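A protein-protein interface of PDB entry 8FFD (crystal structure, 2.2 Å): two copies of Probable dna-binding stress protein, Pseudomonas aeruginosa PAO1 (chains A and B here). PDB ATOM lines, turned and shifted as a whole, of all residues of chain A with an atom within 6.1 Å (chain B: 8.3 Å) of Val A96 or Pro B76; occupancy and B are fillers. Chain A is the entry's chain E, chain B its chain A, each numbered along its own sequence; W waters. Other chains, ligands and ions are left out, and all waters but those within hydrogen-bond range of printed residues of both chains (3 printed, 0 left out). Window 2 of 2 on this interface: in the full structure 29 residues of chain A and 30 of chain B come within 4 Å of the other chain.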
ATOM      1  N   ASN A  35      20.176 -17.585 -18.550  1.00  0.00           N
ATOM      2  CA  ASN A  35      21.398 -16.838 -18.290  1.00  0.00           C
ATOM      3  C   ASN A  35      22.530 -17.272 -19.216  1.00  0.00           C
ATOM      4  O   ASN A  35      23.187 -16.442 -19.852  1.00  0.00           O
ATOM      5  CB  ASN A  35      21.762 -17.045 -16.819  1.00  0.00           C
ATOM      6  CG  ASN A  35      23.078 -16.402 -16.413  1.00  0.00           C
ATOM      7  OD1 ASN A  35      24.020 -16.305 -17.196  1.00  0.00           O
ATOM      8  ND2 ASN A  35      23.159 -16.003 -15.158  1.00  0.00           N
ATOM      9  N   ASN A  39      24.844 -15.366 -22.207  1.00  0.00           N
ATOM     10  CA  ASN A  39      26.168 -14.970 -21.754  1.00  0.00           C
ATOM     11  C   ASN A  39      27.305 -15.828 -22.286  1.00  0.00           C
ATOM     12  O   ASN A  39      28.457 -15.428 -22.136  1.00  0.00           O
ATOM     13  CB  ASN A  39      26.203 -14.970 -20.218  1.00  0.00           C
ATOM     14  CG  ASN A  39      25.531 -13.741 -19.628  1.00  0.00           C
ATOM     15  OD1 ASN A  39      25.902 -12.597 -19.927  1.00  0.00           O
ATOM     16  ND2 ASN A  39      24.523 -13.965 -18.822  1.00  0.00           N
ATOM     17  N   VAL A  40      27.011 -16.984 -22.896  1.00  0.00           N
ATOM     18  CA  VAL A  40      28.041 -17.875 -23.419  1.00  0.00           C
ATOM     19  C   VAL A  40      28.778 -17.195 -24.570  1.00  0.00           C
ATOM     20  O   VAL A  40      28.187 -16.437 -25.354  1.00  0.00           O
ATOM     21  CB  VAL A  40      27.407 -19.210 -23.859  1.00  0.00           C
ATOM     22  CG1 VAL A  40      26.509 -19.021 -25.112  1.00  0.00           C
ATOM     23  CG2 VAL A  40      28.468 -20.270 -24.122  1.00  0.00           C
ATOM     24  N   GLU A  93      24.693 -19.796 -10.310  1.00  0.00           N
ATOM     25  CA  GLU A  93      25.958 -19.314 -10.849  1.00  0.00           C
ATOM     26  C   GLU A  93      25.798 -17.813 -10.985  1.00  0.00           C
ATOM     27  O   GLU A  93      24.983 -17.355 -11.793  1.00  0.00           O
ATOM     28  CB  GLU A  93      26.269 -19.982 -12.191  1.00  0.00           C
ATOM     29  CG  GLU A  93      27.454 -19.401 -12.942  1.00  0.00           C
ATOM     30  CD  GLU A  93      28.713 -19.376 -12.097  1.00  0.00           C
ATOM     31  OE1 GLU A  93      29.208 -20.473 -11.764  1.00  0.00           O
ATOM     32  OE2 GLU A  93      29.181 -18.265 -11.745  1.00  0.00           O
ATOM     33  N   GLU A  94      26.524 -17.058 -10.151  1.00  0.00           N
ATOM     34  CA  GLU A  94      26.462 -15.602 -10.172  1.00  0.00           C
ATOM     35  C   GLU A  94      27.446 -14.978 -11.160  1.00  0.00           C
ATOM     36  O   GLU A  94      27.383 -13.769 -11.385  1.00  0.00           O
ATOM     37  CB  GLU A  94      26.722 -15.022  -8.768  1.00  0.00           C
ATOM     38  CG  GLU A  94      25.823 -15.597  -7.655  1.00  0.00           C
ATOM     39  CD  GLU A  94      24.330 -15.191  -7.748  1.00  0.00           C
ATOM     40  OE1 GLU A  94      23.985 -14.113  -8.284  1.00  0.00           O
ATOM     41  OE2 GLU A  94      23.498 -15.969  -7.257  1.00  0.00           O
ATOM     42  N   GLY A  95      28.331 -15.759 -11.768  1.00  0.00           N
ATOM     43  CA  GLY A  95      29.304 -15.187 -12.674  1.00  0.00           C
ATOM     44  C   GLY A  95      29.116 -15.639 -14.102  1.00  0.00           C
ATOM     45  O   GLY A  95      27.996 -15.950 -14.522  1.00  0.00           O
ATOM     46  N   VAL A  96      30.205 -15.671 -14.863  1.00  0.00           N
ATOM     47  CA  VAL A  96      30.153 -16.104 -16.254  1.00  0.00           C
ATOM     48  C   VAL A  96      31.162 -17.219 -16.498  1.00  0.00           C
ATOM     49  O   VAL A  96      32.297 -16.942 -16.897  1.00  0.00           O
ATOM     50  CB  VAL A  96      30.396 -14.914 -17.196  1.00  0.00           C
ATOM     51  CG1 VAL A  96      30.126 -15.318 -18.651  1.00  0.00           C
ATOM     52  CG2 VAL A  96      29.501 -13.738 -16.796  1.00  0.00           C
ATOM     53  N   PRO A  97      30.801 -18.485 -16.300  1.00  0.00           N
ATOM     54  CA  PRO A  97      31.755 -19.568 -16.555  1.00  0.00           C
ATOM     55  C   PRO A  97      32.138 -19.686 -18.028  1.00  0.00           C
ATOM     56  O   PRO A  97      31.432 -19.231 -18.933  1.00  0.00           O
ATOM     57  CB  PRO A  97      31.010 -20.827 -16.086  1.00  0.00           C
ATOM     58  CG  PRO A  97      29.769 -20.345 -15.431  1.00  0.00           C
ATOM     59  CD  PRO A  97      29.478 -18.996 -15.912  1.00  0.00           C
ATOM     60  N   GLU A  98      33.296 -20.311 -18.254  1.00  0.00           N
ATOM     61  CA  GLU A  98      33.647 -20.772 -19.589  1.00  0.00           C
ATOM     62  C   GLU A  98      32.554 -21.690 -20.138  1.00  0.00           C
ATOM     63  O   GLU A  98      31.801 -22.324 -19.388  1.00  0.00           O
ATOM     64  CB  GLU A  98      34.992 -21.511 -19.545  1.00  0.00           C
ATOM     65  N   MET A 102      29.694 -24.102 -18.294  1.00  0.00           N
ATOM     66  CA  MET A 102      28.247 -23.982 -18.501  1.00  0.00           C
ATOM     67  C   MET A 102      27.632 -25.329 -18.875  1.00  0.00           C
ATOM     68  O   MET A 102      26.640 -25.758 -18.271  1.00  0.00           O
ATOM     69  CB  MET A 102      27.929 -22.934 -19.579  1.00  0.00           C
ATOM     70  CG  MET A 102      28.191 -21.477 -19.142  1.00  0.00           C
ATOM     71  SD  MET A 102      27.812 -20.282 -20.478  1.00  0.00           S
ATOM     72  CE  MET A 102      28.210 -18.750 -19.662  1.00  0.00           C
ATOM     73  N   ALA B  16      24.653  -0.107 -19.695  1.00  0.00           N
ATOM     74  CA  ALA B  16      24.352  -1.479 -19.309  1.00  0.00           C
ATOM     75  C   ALA B  16      23.819  -1.541 -17.884  1.00  0.00           C
ATOM     76  O   ALA B  16      22.926  -2.348 -17.594  1.00  0.00           O
ATOM     77  CB  ALA B  16      25.581  -2.384 -19.449  1.00  0.00           C
ATOM     78  N   GLU B  17      24.330  -0.684 -16.985  1.00  0.00           N
ATOM     79  CA  GLU B  17      23.850  -0.701 -15.597  1.00  0.00           C
ATOM     80  C   GLU B  17      22.375  -0.316 -15.523  1.00  0.00           C
ATOM     81  O   GLU B  17      21.594  -0.968 -14.827  1.00  0.00           O
ATOM     82  CB  GLU B  17      24.712   0.219 -14.719  1.00  0.00           C
ATOM     83  CG  GLU B  17      24.250   0.333 -13.243  1.00  0.00           C
ATOM     84  CD  GLU B  17      22.995   1.233 -13.023  1.00  0.00           C
ATOM     85  OE1 GLU B  17      22.843   2.282 -13.704  1.00  0.00           O
ATOM     86  OE2 GLU B  17      22.154   0.891 -12.158  1.00  0.00           O
ATOM     87  N   LEU B  19      20.162  -0.646 -17.958  1.00  0.00           N
ATOM     88  CA  LEU B  19      19.428  -1.748 -18.558  1.00  0.00           C
ATOM     89  C   LEU B  19      19.379  -2.945 -17.627  1.00  0.00           C
ATOM     90  O   LEU B  19      18.474  -3.773 -17.740  1.00  0.00           O
ATOM     91  CB  LEU B  19      20.059  -2.160 -19.894  1.00  0.00           C
ATOM     92  CG  LEU B  19      19.905  -1.139 -21.034  1.00  0.00           C
ATOM     93  CD1 LEU B  19      20.444  -1.664 -22.344  1.00  0.00           C
ATOM     94  CD2 LEU B  19      18.472  -0.771 -21.230  1.00  0.00           C
ATOM     95  N   SER B  20      20.356  -3.084 -16.730  1.00  0.00           N
ATOM     96  CA  SER B  20      20.314  -4.216 -15.808  1.00  0.00           C
ATOM     97  C   SER B  20      19.185  -4.036 -14.800  1.00  0.00           C
ATOM     98  O   SER B  20      18.508  -5.006 -14.439  1.00  0.00           O
ATOM     99  CB  SER B  20      21.657  -4.375 -15.088  1.00  0.00           C
ATOM    100  OG  SER B  20      22.653  -4.836 -15.993  1.00  0.00           O
ATOM    101  N   LEU B  23      16.098  -4.739 -16.737  1.00  0.00           N
ATOM    102  CA  LEU B  23      15.951  -6.183 -16.824  1.00  0.00           C
ATOM    103  C   LEU B  23      15.368  -6.729 -15.527  1.00  0.00           C
ATOM    104  O   LEU B  23      14.396  -7.496 -15.537  1.00  0.00           O
ATOM    105  CB  LEU B  23      17.311  -6.826 -17.149  1.00  0.00           C
ATOM    106  CG  LEU B  23      17.322  -8.361 -17.215  1.00  0.00           C
ATOM    107  CD1 LEU B  23      16.202  -8.835 -18.126  1.00  0.00           C
ATOM    108  CD2 LEU B  23      18.642  -8.917 -17.727  1.00  0.00           C
ATOM    109  N   ILE B  66      15.891  -7.210 -23.731  1.00  0.00           N
ATOM    110  CA  ILE B  66      16.706  -6.353 -22.860  1.00  0.00           C
ATOM    111  C   ILE B  66      18.055  -7.004 -22.553  1.00  0.00           C
ATOM    112  O   ILE B  66      19.106  -6.350 -22.592  1.00  0.00           O
ATOM    113  CB  ILE B  66      15.948  -6.025 -21.562  1.00  0.00           C
ATOM    114  CG1 ILE B  66      14.663  -5.243 -21.847  1.00  0.00           C
ATOM    115  CG2 ILE B  66      16.819  -5.190 -20.627  1.00  0.00           C
ATOM    116  CD1 ILE B  66      13.660  -5.269 -20.636  1.00  0.00           C
ATOM    117  N   ALA B  67      18.052  -8.295 -22.239  1.00  0.00           N
ATOM    118  CA  ALA B  67      19.309  -8.959 -21.939  1.00  0.00           C
ATOM    119  C   ALA B  67      20.268  -8.865 -23.118  1.00  0.00           C
ATOM    120  O   ALA B  67      21.460  -8.612 -22.932  1.00  0.00           O
ATOM    121  CB  ALA B  67      19.062 -10.419 -21.559  1.00  0.00           C
ATOM    122  N   ARG B  69      20.366  -6.592 -25.506  1.00  0.00           N
ATOM    123  CA  ARG B  69      20.930  -5.262 -25.688  1.00  0.00           C
ATOM    124  C   ARG B  69      22.128  -5.071 -24.772  1.00  0.00           C
ATOM    125  O   ARG B  69      23.150  -4.509 -25.177  1.00  0.00           O
ATOM    126  CB  ARG B  69      19.889  -4.182 -25.431  1.00  0.00           C
ATOM    127  CG  ARG B  69      20.424  -2.787 -25.714  1.00  0.00           C
ATOM    128  CD  ARG B  69      20.709  -2.550 -27.218  1.00  0.00           C
ATOM    129  NE  ARG B  69      21.389  -1.272 -27.414  1.00  0.00           N
ATOM    130  CZ  ARG B  69      22.344  -1.068 -28.305  1.00  0.00           C
ATOM    131  NH1 ARG B  69      22.718  -2.024 -29.140  1.00  0.00           N
ATOM    132  NH2 ARG B  69      22.950   0.116 -28.352  1.00  0.00           N
ATOM    133  N   ILE B  70      22.041  -5.589 -23.547  1.00  0.00           N
ATOM    134  CA  ILE B  70      23.171  -5.507 -22.635  1.00  0.00           C
ATOM    135  C   ILE B  70      24.387  -6.199 -23.250  1.00  0.00           C
ATOM    136  O   ILE B  70      25.515  -5.699 -23.165  1.00  0.00           O
ATOM    137  CB  ILE B  70      22.783  -6.104 -21.262  1.00  0.00           C
ATOM    138  CG1 ILE B  70      21.719  -5.258 -20.574  1.00  0.00           C
ATOM    139  CG2 ILE B  70      23.971  -6.178 -20.366  1.00  0.00           C
ATOM    140  CD1 ILE B  70      21.124  -5.892 -19.299  1.00  0.00           C
ATOM    141  N   ARG B  71      24.176  -7.353 -23.893  1.00  0.00           N
ATOM    142  CA  ARG B  71      25.287  -8.062 -24.536  1.00  0.00           C
ATOM    143  C   ARG B  71      25.837  -7.262 -25.722  1.00  0.00           C
ATOM    144  O   ARG B  71      27.050  -7.186 -25.919  1.00  0.00           O
ATOM    145  CB  ARG B  71      24.833  -9.457 -24.988  1.00  0.00           C
ATOM    146  CG  ARG B  71      24.311 -10.367 -23.894  1.00  0.00           C
ATOM    147  CD  ARG B  71      25.356 -10.635 -22.825  1.00  0.00           C
ATOM    148  NE  ARG B  71      26.434 -11.451 -23.362  1.00  0.00           N
ATOM    149  CZ  ARG B  71      27.677 -11.031 -23.569  1.00  0.00           C
ATOM    150  NH1 ARG B  71      28.096  -9.845 -23.144  1.00  0.00           N
ATOM    151  NH2 ARG B  71      28.527 -11.823 -24.212  1.00  0.00           N
ATOM    152  N   ALA B  72      24.956  -6.649 -26.514  1.00  0.00           N
ATOM    153  CA  ALA B  72      25.411  -5.806 -27.605  1.00  0.00           C
ATOM    154  C   ALA B  72      26.258  -4.639 -27.117  1.00  0.00           C
ATOM    155  O   ALA B  72      27.182  -4.219 -27.820  1.00  0.00           O
ATOM    156  CB  ALA B  72      24.212  -5.296 -28.391  1.00  0.00           C
ATOM    157  N   LEU B  73      25.964  -4.092 -25.934  1.00  0.00           N
ATOM    158  CA  LEU B  73      26.812  -3.042 -25.374  1.00  0.00           C
ATOM    159  C   LEU B  73      28.112  -3.586 -24.780  1.00  0.00           C
ATOM    160  O   LEU B  73      28.984  -2.805 -24.393  1.00  0.00           O
ATOM    161  CB  LEU B  73      26.042  -2.245 -24.312  1.00  0.00           C
ATOM    162  CG  LEU B  73      24.832  -1.455 -24.826  1.00  0.00           C
ATOM    163  CD1 LEU B  73      23.915  -1.075 -23.688  1.00  0.00           C
ATOM    164  CD2 LEU B  73      25.262  -0.213 -25.551  1.00  0.00           C
ATOM    165  N   GLY B  74      28.291  -4.892 -24.720  1.00  0.00           N
ATOM    166  CA  GLY B  74      29.555  -5.441 -24.294  1.00  0.00           C
ATOM    167  C   GLY B  74      29.649  -5.851 -22.844  1.00  0.00           C
ATOM    168  O   GLY B  74      30.765  -5.918 -22.312  1.00  0.00           O
ATOM    169  N   PHE B  75      28.536  -6.142 -22.194  1.00  0.00           N
ATOM    170  CA  PHE B  75      28.543  -6.490 -20.784  1.00  0.00           C
ATOM    171  C   PHE B  75      27.680  -7.707 -20.519  1.00  0.00           C
ATOM    172  O   PHE B  75      26.807  -8.049 -21.327  1.00  0.00           O
ATOM    173  CB  PHE B  75      28.082  -5.293 -19.949  1.00  0.00           C
ATOM    174  CG  PHE B  75      29.047  -4.180 -20.000  1.00  0.00           C
ATOM    175  CD1 PHE B  75      29.016  -3.269 -21.042  1.00  0.00           C
ATOM    176  CD2 PHE B  75      30.049  -4.071 -19.054  1.00  0.00           C
ATOM    177  CE1 PHE B  75      29.940  -2.222 -21.117  1.00  0.00           C
ATOM    178  CE2 PHE B  75      30.975  -3.030 -19.124  1.00  0.00           C
ATOM    179  CZ  PHE B  75      30.916  -2.112 -20.165  1.00  0.00           C
ATOM    180  N   PRO B  76      27.949  -8.421 -19.422  1.00  0.00           N
ATOM    181  CA  PRO B  76      27.203  -9.640 -19.131  1.00  0.00           C
ATOM    182  C   PRO B  76      25.825  -9.309 -18.593  1.00  0.00           C
ATOM    183  O   PRO B  76      25.600  -8.270 -17.972  1.00  0.00           O
ATOM    184  CB  PRO B  76      28.074 -10.353 -18.085  1.00  0.00           C
ATOM    185  CG  PRO B  76      28.832  -9.279 -17.412  1.00  0.00           C
ATOM    186  CD  PRO B  76      28.989  -8.147 -18.406  1.00  0.00           C
ATOM    187  N   ALA B  77      24.877 -10.185 -18.896  1.00  0.00           N
ATOM    188  CA  ALA B  77      23.501  -9.926 -18.531  1.00  0.00           C
ATOM    189  C   ALA B  77      23.238 -10.612 -17.202  1.00  0.00           C
ATOM    190  O   ALA B  77      23.459 -11.826 -17.098  1.00  0.00           O
ATOM    191  CB  ALA B  77      22.544 -10.445 -19.591  1.00  0.00           C
ATOM    192  N   PRO B  78      22.814  -9.889 -16.165  1.00  0.00           N
ATOM    193  CA  PRO B  78      22.470 -10.549 -14.891  1.00  0.00           C
ATOM    194  C   PRO B  78      21.305 -11.515 -15.056  1.00  0.00           C
ATOM    195  O   PRO B  78      20.450 -11.353 -15.935  1.00  0.00           O
ATOM    196  CB  PRO B  78      22.105  -9.384 -13.962  1.00  0.00           C
ATOM    197  CG  PRO B  78      21.904  -8.176 -14.859  1.00  0.00           C
ATOM    198  CD  PRO B  78      22.478  -8.455 -16.197  1.00  0.00           C
ATOM    199  N   GLY B  79      21.295 -12.547 -14.211  1.00  0.00           N
ATOM    200  CA  GLY B  79      20.367 -13.657 -14.383  1.00  0.00           C
ATOM    201  C   GLY B  79      20.328 -14.689 -13.263  1.00  0.00           C
ATOM    202  O   GLY B  79      20.452 -15.900 -13.503  1.00  0.00           O
HETATM  203  O   HOH W   1      28.420 -12.918 -21.149  1.00  0.00           O
HETATM  204  O   HOH W   2      27.014 -14.061 -25.363  1.00  0.00           O
HETATM  205  O   HOH W   3      25.863 -12.793 -15.990  1.00  0.00           O
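Water W2 lies within hydrogen-bond range of O of Val A40 (2.6 Å) and NH2 of Arg B71 (2.9 Å).
Water W1 bridges the backbone carbonyl oxygen (O) of Asn A39 (2.7 Å) and the guanidinium group (NH2) of Arg B71 (3.3 Å).
Water W3 lies within hydrogen-bond range of the backbone carbonyl oxygen (O) of Ala B77 (2.8 Å) and the side-chain amide nitrogen (ND2) of Asn A39 (3.3 Å).
Printed residues of chain B that touch a printed residue of chain A: Arg B71, Pro B76, Ala B77 and Gly B79.
Hydrophobic or aromatic side chains of chain B that line the printed part of chain A: Pro B76.
Hydrophobic or aromatic side chains of chain A that line the printed part of chain B: Val A96.
Among the printed residues, 5 pairs touch across the chains.
Among the printed residues, no Asp or Glu carboxylate lies within 4 Å of a Lys or Arg side-chain nitrogen of the other chain.
Printed residues of chain B within 4 Å of Asn A35: Gly B79.
No residue of chain B comes within 4 Å of Gly A95.
Val A96 touches just one residue of chain B: Pro B76 (3.9 Å).
Pro A97 touches none of the printed residues of chain B.
Ala B67 touches none of the printed residues of chain A.
Printed residues of chain A within 4 Å of Arg B71: Asn A39.
Ala B72 touches none of the printed residues of chain A.
Pro B76 touches just these residues of chain A: Asn A39 (3.3 Å) and Val A96 (3.9 Å).
Printed residues of chain A within 4 Å of Gly B79: Asn A35 (3.2 Å).
The nearest residue of chain B that does not touch Val A96 is Ala B77 (6.2 Å).
The nearest printed residue of chain A that does not touch Pro B76 is Gly A95 (6.6 Å).
NH1 of Arg B71 is in hydrogen-bond range of O of Phe B75 (2.9 Å).
The side-chain amide oxygen of Asn A35 lies within hydrogen-bond range of the side-chain amide nitrogen of Asn A39 (2.9 Å).
The backbone NH of Ala B77 sits at hydrogen-bond distance from the side-chain amide oxygen of Asn A39, 2.8 Å away.
The backbone carbonyl oxygen of Gly B79 is in hydrogen-bond range of the side-chain amide nitrogen of Asn A35 (3.2 Å).
Arg B71 touches Asn A39.
OD1 of Asn A39 touches CA of Pro B76, at 3.3 Å.
CG2 of Val A96 touches CB of Pro B76 (3.9 Å).
No position is printed for both chains.
Of the 5 pairs that touch across the chains among the printed residues, none has its exchanged pair printed and touching as well.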
